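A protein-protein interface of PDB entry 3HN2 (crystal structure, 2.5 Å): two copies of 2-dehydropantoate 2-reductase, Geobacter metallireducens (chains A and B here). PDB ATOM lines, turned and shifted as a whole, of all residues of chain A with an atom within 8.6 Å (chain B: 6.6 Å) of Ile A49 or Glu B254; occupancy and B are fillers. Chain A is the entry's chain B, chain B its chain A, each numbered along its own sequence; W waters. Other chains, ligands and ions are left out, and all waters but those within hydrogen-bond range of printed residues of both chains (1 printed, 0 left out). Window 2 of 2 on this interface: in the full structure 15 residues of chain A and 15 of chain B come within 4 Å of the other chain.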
ATOM      1  N   TYR A  16     -15.176 -10.261  15.258  1.00  0.00           N
ATOM      2  CA  TYR A  16     -15.265  -8.809  15.480  1.00  0.00           C
ATOM      3  C   TYR A  16     -14.693  -7.979  14.333  1.00  0.00           C
ATOM      4  O   TYR A  16     -15.354  -7.065  13.840  1.00  0.00           O
ATOM      5  CB  TYR A  16     -14.596  -8.399  16.798  1.00  0.00           C
ATOM      6  CG  TYR A  16     -14.648  -6.908  17.075  1.00  0.00           C
ATOM      7  CD1 TYR A  16     -15.860  -6.276  17.350  1.00  0.00           C
ATOM      8  CD2 TYR A  16     -13.487  -6.131  17.068  1.00  0.00           C
ATOM      9  CE1 TYR A  16     -15.925  -4.914  17.600  1.00  0.00           C
ATOM     10  CE2 TYR A  16     -13.542  -4.761  17.319  1.00  0.00           C
ATOM     11  CZ  TYR A  16     -14.767  -4.162  17.589  1.00  0.00           C
ATOM     12  OH  TYR A  16     -14.854  -2.811  17.841  1.00  0.00           O
ATOM     13  N   VAL A  46     -23.294  -8.098  16.892  1.00  0.00           N
ATOM     14  CA  VAL A  46     -22.159  -7.475  17.565  1.00  0.00           C
ATOM     15  C   VAL A  46     -22.682  -6.582  18.678  1.00  0.00           C
ATOM     16  O   VAL A  46     -23.424  -5.630  18.427  1.00  0.00           O
ATOM     17  CB  VAL A  46     -21.276  -6.648  16.597  1.00  0.00           C
ATOM     18  CG1 VAL A  46     -20.139  -5.950  17.349  1.00  0.00           C
ATOM     19  CG2 VAL A  46     -20.718  -7.532  15.512  1.00  0.00           C
ATOM     20  N   PHE A  47     -22.306  -6.913  19.907  1.00  0.00           N
ATOM     21  CA  PHE A  47     -22.611  -6.083  21.061  1.00  0.00           C
ATOM     22  C   PHE A  47     -21.352  -5.299  21.425  1.00  0.00           C
ATOM     23  O   PHE A  47     -20.368  -5.873  21.894  1.00  0.00           O
ATOM     24  CB  PHE A  47     -23.107  -6.944  22.232  1.00  0.00           C
ATOM     25  CG  PHE A  47     -24.445  -7.601  21.984  1.00  0.00           C
ATOM     26  CD1 PHE A  47     -24.518  -8.894  21.471  1.00  0.00           C
ATOM     27  CD2 PHE A  47     -25.633  -6.922  22.261  1.00  0.00           C
ATOM     28  CE1 PHE A  47     -25.754  -9.503  21.235  1.00  0.00           C
ATOM     29  CE2 PHE A  47     -26.872  -7.521  22.032  1.00  0.00           C
ATOM     30  CZ  PHE A  47     -26.933  -8.813  21.517  1.00  0.00           C
ATOM     31  N   SER A  48     -21.377  -3.991  21.184  1.00  0.00           N
ATOM     32  CA  SER A  48     -20.184  -3.166  21.354  1.00  0.00           C
ATOM     33  C   SER A  48     -20.382  -1.996  22.311  1.00  0.00           C
ATOM     34  O   SER A  48     -21.507  -1.555  22.548  1.00  0.00           O
ATOM     35  CB  SER A  48     -19.699  -2.656  19.993  1.00  0.00           C
ATOM     36  OG  SER A  48     -18.525  -1.874  20.128  1.00  0.00           O
ATOM     37  N   ILE A  49     -19.274  -1.502  22.860  1.00  0.00           N
ATOM     38  CA  ILE A  49     -19.286  -0.275  23.653  1.00  0.00           C
ATOM     39  C   ILE A  49     -19.329   0.961  22.748  1.00  0.00           C
ATOM     40  O   ILE A  49     -19.688   2.053  23.194  1.00  0.00           O
ATOM     41  CB  ILE A  49     -18.092  -0.183  24.643  1.00  0.00           C
ATOM     42  CG1 ILE A  49     -16.755  -0.395  23.923  1.00  0.00           C
ATOM     43  CG2 ILE A  49     -18.278  -1.167  25.800  1.00  0.00           C
ATOM     44  CD1 ILE A  49     -15.565   0.116  24.692  1.00  0.00           C
ATOM     45  N   ASN A  50     -18.960   0.778  21.481  1.00  0.00           N
ATOM     46  CA  ASN A  50     -19.114   1.810  20.457  1.00  0.00           C
ATOM     47  C   ASN A  50     -20.416   1.622  19.661  1.00  0.00           C
ATOM     48  O   ASN A  50     -20.457   1.850  18.448  1.00  0.00           O
ATOM     49  CB  ASN A  50     -17.901   1.823  19.515  1.00  0.00           C
ATOM     50  CG  ASN A  50     -16.600   2.197  20.221  1.00  0.00           C
ATOM     51  OD1 ASN A  50     -16.593   2.600  21.383  1.00  0.00           O
ATOM     52  ND2 ASN A  50     -15.488   2.063  19.508  1.00  0.00           N
ATOM     53  N   GLY A  51     -21.473   1.199  20.353  1.00  0.00           N
ATOM     54  CA  GLY A  51     -22.781   0.975  19.742  1.00  0.00           C
ATOM     55  C   GLY A  51     -22.920  -0.399  19.114  1.00  0.00           C
ATOM     56  O   GLY A  51     -22.060  -0.824  18.336  1.00  0.00           O
ATOM     57  N   ASP A  52     -24.009  -1.087  19.451  1.00  0.00           N
ATOM     58  CA  ASP A  52     -24.304  -2.412  18.904  1.00  0.00           C
ATOM     59  C   ASP A  52     -24.751  -2.316  17.450  1.00  0.00           C
ATOM     60  O   ASP A  52     -25.318  -1.301  17.034  1.00  0.00           O
ATOM     61  CB  ASP A  52     -25.407  -3.113  19.709  1.00  0.00           C
ATOM     62  CG  ASP A  52     -25.131  -3.143  21.202  1.00  0.00           C
ATOM     63  OD1 ASP A  52     -26.101  -3.316  21.969  1.00  0.00           O
ATOM     64  OD2 ASP A  52     -23.962  -2.997  21.615  1.00  0.00           O
ATOM     65  N   PHE A  53     -24.481  -3.372  16.686  1.00  0.00           N
ATOM     66  CA  PHE A  53     -25.036  -3.537  15.343  1.00  0.00           C
ATOM     67  C   PHE A  53     -25.162  -5.022  14.999  1.00  0.00           C
ATOM     68  O   PHE A  53     -24.403  -5.851  15.504  1.00  0.00           O
ATOM     69  CB  PHE A  53     -24.226  -2.765  14.284  1.00  0.00           C
ATOM     70  CG  PHE A  53     -22.913  -3.402  13.916  1.00  0.00           C
ATOM     71  CD1 PHE A  53     -21.777  -3.193  14.695  1.00  0.00           C
ATOM     72  CD2 PHE A  53     -22.802  -4.184  12.765  1.00  0.00           C
ATOM     73  CE1 PHE A  53     -20.559  -3.772  14.348  1.00  0.00           C
ATOM     74  CE2 PHE A  53     -21.589  -4.771  12.414  1.00  0.00           C
ATOM     75  CZ  PHE A  53     -20.465  -4.563  13.206  1.00  0.00           C
ATOM     76  N   LEU A 128      -7.291  -6.157  21.932  1.00  0.00           N
ATOM     77  CA  LEU A 128      -8.741  -6.287  21.916  1.00  0.00           C
ATOM     78  C   LEU A 128      -9.288  -6.869  23.217  1.00  0.00           C
ATOM     79  O   LEU A 128      -8.899  -7.964  23.630  1.00  0.00           O
ATOM     80  CB  LEU A 128      -9.166  -7.173  20.742  1.00  0.00           C
ATOM     81  CG  LEU A 128     -10.368  -6.843  19.845  1.00  0.00           C
ATOM     82  CD1 LEU A 128     -10.894  -8.133  19.237  1.00  0.00           C
ATOM     83  CD2 LEU A 128     -11.498  -6.101  20.552  1.00  0.00           C
ATOM     84  N   CYS A 129     -10.198  -6.130  23.847  1.00  0.00           N
ATOM     85  CA  CYS A 129     -10.932  -6.620  25.011  1.00  0.00           C
ATOM     86  C   CYS A 129     -12.268  -7.190  24.549  1.00  0.00           C
ATOM     87  O   CYS A 129     -13.203  -6.438  24.256  1.00  0.00           O
ATOM     88  CB  CYS A 129     -11.163  -5.500  26.031  1.00  0.00           C
ATOM     89  SG  CYS A 129      -9.694  -4.553  26.474  1.00  0.00           S
ATOM     90  N   VAL A 138     -20.920 -11.579  19.523  1.00  0.00           N
ATOM     91  CA  VAL A 138     -19.603 -11.031  19.878  1.00  0.00           C
ATOM     92  C   VAL A 138     -19.783  -9.888  20.872  1.00  0.00           C
ATOM     93  O   VAL A 138     -20.637  -9.025  20.671  1.00  0.00           O
ATOM     94  CB  VAL A 138     -18.823 -10.501  18.637  1.00  0.00           C
ATOM     95  CG1 VAL A 138     -17.352 -10.273  18.974  1.00  0.00           C
ATOM     96  CG2 VAL A 138     -18.935 -11.458  17.466  1.00  0.00           C
ATOM     97  N   HIS A 139     -18.980  -9.884  21.936  1.00  0.00           N
ATOM     98  CA  HIS A 139     -19.029  -8.814  22.937  1.00  0.00           C
ATOM     99  C   HIS A 139     -17.751  -7.968  22.981  1.00  0.00           C
ATOM    100  O   HIS A 139     -16.755  -8.357  23.593  1.00  0.00           O
ATOM    101  CB  HIS A 139     -19.343  -9.375  24.329  1.00  0.00           C
ATOM    102  CG  HIS A 139     -20.665 -10.067  24.420  1.00  0.00           C
ATOM    103  ND1 HIS A 139     -20.813 -11.416  24.181  1.00  0.00           N
ATOM    104  CD2 HIS A 139     -21.898  -9.601  24.725  1.00  0.00           C
ATOM    105  CE1 HIS A 139     -22.082 -11.751  24.331  1.00  0.00           C
ATOM    106  NE2 HIS A 139     -22.762 -10.667  24.663  1.00  0.00           N
ATOM    107  N   HIS A 140     -17.801  -6.807  22.333  1.00  0.00           N
ATOM    108  CA  HIS A 140     -16.709  -5.839  22.355  1.00  0.00           C
ATOM    109  C   HIS A 140     -16.753  -5.063  23.671  1.00  0.00           C
ATOM    110  O   HIS A 140     -17.754  -4.413  23.991  1.00  0.00           O
ATOM    111  CB  HIS A 140     -16.823  -4.901  21.150  1.00  0.00           C
ATOM    112  CG  HIS A 140     -15.758  -3.851  21.085  1.00  0.00           C
ATOM    113  ND1 HIS A 140     -16.044  -2.503  21.054  1.00  0.00           N
ATOM    114  CD2 HIS A 140     -14.408  -3.950  21.037  1.00  0.00           C
ATOM    115  CE1 HIS A 140     -14.917  -1.815  20.992  1.00  0.00           C
ATOM    116  NE2 HIS A 140     -13.910  -2.669  20.981  1.00  0.00           N
ATOM    117  N   LEU A 141     -15.667  -5.146  24.434  1.00  0.00           N
ATOM    118  CA  LEU A 141     -15.618  -4.555  25.767  1.00  0.00           C
ATOM    119  C   LEU A 141     -14.658  -3.375  25.870  1.00  0.00           C
ATOM    120  O   LEU A 141     -14.757  -2.568  26.799  1.00  0.00           O
ATOM    121  CB  LEU A 141     -15.251  -5.614  26.814  1.00  0.00           C
ATOM    122  CG  LEU A 141     -16.198  -6.787  27.088  1.00  0.00           C
ATOM    123  CD1 LEU A 141     -15.748  -7.527  28.341  1.00  0.00           C
ATOM    124  CD2 LEU A 141     -17.655  -6.342  27.212  1.00  0.00           C
ATOM    125  N   GLY A 142     -13.730  -3.280  24.920  1.00  0.00           N
ATOM    126  CA  GLY A 142     -12.715  -2.233  24.950  1.00  0.00           C
ATOM    127  C   GLY A 142     -11.704  -2.281  23.823  1.00  0.00           C
ATOM    128  O   GLY A 142     -11.488  -3.333  23.207  1.00  0.00           O
ATOM    129  N   ALA A 143     -11.095  -1.119  23.573  1.00  0.00           N
ATOM    130  CA  ALA A 143     -10.024  -0.923  22.588  1.00  0.00           C
ATOM    131  C   ALA A 143     -10.328  -1.513  21.204  1.00  0.00           C
ATOM    132  O   ALA A 143     -11.458  -1.415  20.720  1.00  0.00           O
ATOM    133  CB  ALA A 143      -8.684  -1.428  23.139  1.00  0.00           C
ATOM    134  N   GLY A 144      -9.322  -2.118  20.578  1.00  0.00           N
ATOM    135  CA  GLY A 144      -9.487  -2.745  19.274  1.00  0.00           C
ATOM    136  C   GLY A 144      -8.377  -2.427  18.295  1.00  0.00           C
ATOM    137  O   GLY A 144      -8.369  -2.954  17.185  1.00  0.00           O
ATOM    138  N   ALA A 251      -5.852   0.745  34.911  1.00  0.00           N
ATOM    139  CA  ALA A 251      -7.103   1.378  34.505  1.00  0.00           C
ATOM    140  C   ALA A 251      -7.986   0.459  33.651  1.00  0.00           C
ATOM    141  O   ALA A 251      -8.832   0.931  32.887  1.00  0.00           O
ATOM    142  CB  ALA A 251      -6.818   2.677  33.776  1.00  0.00           C
ATOM    143  N   PRO B 203     -19.563   8.598  27.153  1.00  0.00           N
ATOM    144  CA  PRO B 203     -18.346   8.048  27.777  1.00  0.00           C
ATOM    145  C   PRO B 203     -17.088   8.166  26.897  1.00  0.00           C
ATOM    146  O   PRO B 203     -17.187   8.508  25.713  1.00  0.00           O
ATOM    147  CB  PRO B 203     -18.705   6.579  28.003  1.00  0.00           C
ATOM    148  CG  PRO B 203     -19.727   6.282  26.961  1.00  0.00           C
ATOM    149  CD  PRO B 203     -20.531   7.536  26.815  1.00  0.00           C
ATOM    150  N   VAL B 204     -15.924   7.869  27.479  1.00  0.00           N
ATOM    151  CA  VAL B 204     -14.618   8.113  26.832  1.00  0.00           C
ATOM    152  C   VAL B 204     -14.368   7.333  25.528  1.00  0.00           C
ATOM    153  O   VAL B 204     -13.714   7.847  24.620  1.00  0.00           O
ATOM    154  CB  VAL B 204     -13.405   7.945  27.818  1.00  0.00           C
ATOM    155  CG1 VAL B 204     -13.502   8.923  28.966  1.00  0.00           C
ATOM    156  CG2 VAL B 204     -13.299   6.525  28.363  1.00  0.00           C
ATOM    157  N   ASN B 205     -14.904   6.118  25.433  1.00  0.00           N
ATOM    158  CA  ASN B 205     -14.711   5.259  24.251  1.00  0.00           C
ATOM    159  C   ASN B 205     -15.251   5.840  22.948  1.00  0.00           C
ATOM    160  O   ASN B 205     -14.693   5.595  21.881  1.00  0.00           O
ATOM    161  CB  ASN B 205     -15.312   3.873  24.477  1.00  0.00           C
ATOM    162  CG  ASN B 205     -16.806   3.914  24.724  1.00  0.00           C
ATOM    163  OD1 ASN B 205     -17.263   4.273  25.806  1.00  0.00           O
ATOM    164  ND2 ASN B 205     -17.578   3.537  23.716  1.00  0.00           N
ATOM    165  N   LEU B 206     -16.330   6.609  23.052  1.00  0.00           N
ATOM    166  CA  LEU B 206     -16.939   7.276  21.913  1.00  0.00           C
ATOM    167  C   LEU B 206     -16.102   8.454  21.424  1.00  0.00           C
ATOM    168  O   LEU B 206     -15.835   8.553  20.222  1.00  0.00           O
ATOM    169  CB  LEU B 206     -18.364   7.721  22.255  1.00  0.00           C
ATOM    170  CG  LEU B 206     -19.378   6.617  22.585  1.00  0.00           C
ATOM    171  CD1 LEU B 206     -20.758   7.214  22.803  1.00  0.00           C
ATOM    172  CD2 LEU B 206     -19.424   5.550  21.497  1.00  0.00           C
ATOM    173  N   MET B 252      -9.816   1.750  29.104  1.00  0.00           N
ATOM    174  CA  MET B 252     -10.778   2.072  30.145  1.00  0.00           C
ATOM    175  C   MET B 252     -12.178   1.676  29.755  1.00  0.00           C
ATOM    176  O   MET B 252     -13.098   1.792  30.566  1.00  0.00           O
ATOM    177  CB  MET B 252     -10.757   3.569  30.441  1.00  0.00           C
ATOM    178  CG  MET B 252      -9.635   4.025  31.341  1.00  0.00           C
ATOM    179  SD  MET B 252      -9.680   5.813  31.413  1.00  0.00           S
ATOM    180  CE  MET B 252      -9.127   6.143  33.092  1.00  0.00           C
ATOM    181  N   GLY B 253     -12.333   1.220  28.511  1.00  0.00           N
ATOM    182  CA  GLY B 253     -13.630   0.842  27.958  1.00  0.00           C
ATOM    183  C   GLY B 253     -14.635   1.977  28.020  1.00  0.00           C
ATOM    184  O   GLY B 253     -14.337   3.106  27.622  1.00  0.00           O
ATOM    185  N   GLU B 254     -15.808   1.673  28.569  1.00  0.00           N
ATOM    186  CA  GLU B 254     -16.946   2.585  28.597  1.00  0.00           C
ATOM    187  C   GLU B 254     -16.987   3.411  29.895  1.00  0.00           C
ATOM    188  O   GLU B 254     -17.942   3.331  30.671  1.00  0.00           O
ATOM    189  CB  GLU B 254     -18.238   1.778  28.406  1.00  0.00           C
ATOM    190  CG  GLU B 254     -19.420   2.565  27.851  1.00  0.00           C
ATOM    191  CD  GLU B 254     -20.687   1.730  27.729  1.00  0.00           C
ATOM    192  OE1 GLU B 254     -21.530   2.061  26.870  1.00  0.00           O
ATOM    193  OE2 GLU B 254     -20.847   0.749  28.487  1.00  0.00           O
ATOM    194  N   TYR B 255     -15.953   4.217  30.118  1.00  0.00           N
ATOM    195  CA  TYR B 255     -15.806   4.940  31.387  1.00  0.00           C
ATOM    196  C   TYR B 255     -16.354   6.365  31.354  1.00  0.00           C
ATOM    197  O   TYR B 255     -16.022   7.153  30.469  1.00  0.00           O
ATOM    198  CB  TYR B 255     -14.344   4.941  31.838  1.00  0.00           C
ATOM    199  CG  TYR B 255     -14.075   5.774  33.072  1.00  0.00           C
ATOM    200  CD1 TYR B 255     -13.288   6.921  32.999  1.00  0.00           C
ATOM    201  CD2 TYR B 255     -14.609   5.417  34.313  1.00  0.00           C
ATOM    202  CE1 TYR B 255     -13.041   7.693  34.121  1.00  0.00           C
ATOM    203  CE2 TYR B 255     -14.369   6.188  35.445  1.00  0.00           C
ATOM    204  CZ  TYR B 255     -13.583   7.324  35.341  1.00  0.00           C
ATOM    205  OH  TYR B 255     -13.328   8.094  36.452  1.00  0.00           O
ATOM    206  N   LYS B 256     -17.189   6.692  32.334  1.00  0.00           N
ATOM    207  CA  LYS B 256     -17.787   8.017  32.421  1.00  0.00           C
ATOM    208  C   LYS B 256     -17.141   8.805  33.558  1.00  0.00           C
ATOM    209  O   LYS B 256     -17.390   8.513  34.730  1.00  0.00           O
ATOM    210  CB  LYS B 256     -19.312   7.924  32.597  1.00  0.00           C
ATOM    211  CG  LYS B 256     -20.011   7.037  31.554  1.00  0.00           C
ATOM    212  CD  LYS B 256     -21.317   7.643  31.051  1.00  0.00           C
ATOM    213  CE  LYS B 256     -22.552   7.034  31.685  1.00  0.00           C
ATOM    214  NZ  LYS B 256     -23.774   7.338  30.870  1.00  0.00           N
HETATM  215  O   HOH W   1     -13.375   3.142  21.237  1.00  0.00           O
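ND2 of Asn B205 is in hydrogen-bond range of O of Ile A49.
The side-chain amide oxygen (OD1) of Asn A50 sits at hydrogen-bond distance from the side-chain amide nitrogen (ND2) of Asn B205, 2.7 Å away.
Printed residues of chain B that touch a printed residue of chain A: Asn B205, Leu B206, Met B252, Gly B253 and Glu B254.
Along chain B the printed residues that touch a printed residue of chain A span positions 205 to 254.
Printed residues of chain A that touch a printed residue of chain B: Ile A49, Asn A50, Leu A141 and Ala A251.
Among the printed residues, merely in contact across the chains: Ile A49 with Leu B206 (3.9 Å), Ile A49 with Gly B253 (3.9 Å), Ile A49 with Glu B254 (3.9 Å), Asn A50 with Leu B206 (3.9 Å), Leu A141 with Gly B253 (3.8 Å) and Ala A251 with Met B252 (3.6 Å).
No position is printed for both chains.
O of Cys A129 is in hydrogen-bond range of N of Leu A141.
The side-chain hydroxyl (OG) of Ser A48 lies within hydrogen-bond range of the backbone NH (N) of Asn A50 (3.0 Å).
O of His A140 is in hydrogen-bond range of N of Ile A49 (3.5 Å).
Ile A49 touches four residues of chain B.
Of chain A, only Ile A49 comes within 4 Å of Glu B254.
Gly B253 touches just these residues of chain A: Ile A49 and Leu A141.
Of the printed residues of chain B, Ala A251 touches Met B252.
Printed residues of chain A within 4 Å of Asn B205: Ile A49 (2.6 Å) and Asn A50 (2.7 Å).
Printed residues of chain A within 4 Å of Met B252: Ala A251 (3.6 Å).
Printed residues of chain B within 4 Å of Asn A50: Asn B205 and Leu B206.
The nearest residue of chain B that does not touch Ile A49 is Pro B203 (5.7 Å).
The nearest residue of chain A that does not touch Glu B254 is Leu A141 (4.7 Å).
Water W1 lies within hydrogen-bond range of O of Asn B205 (2.9 Å) and ND2 of Asn A50 (2.9 Å).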
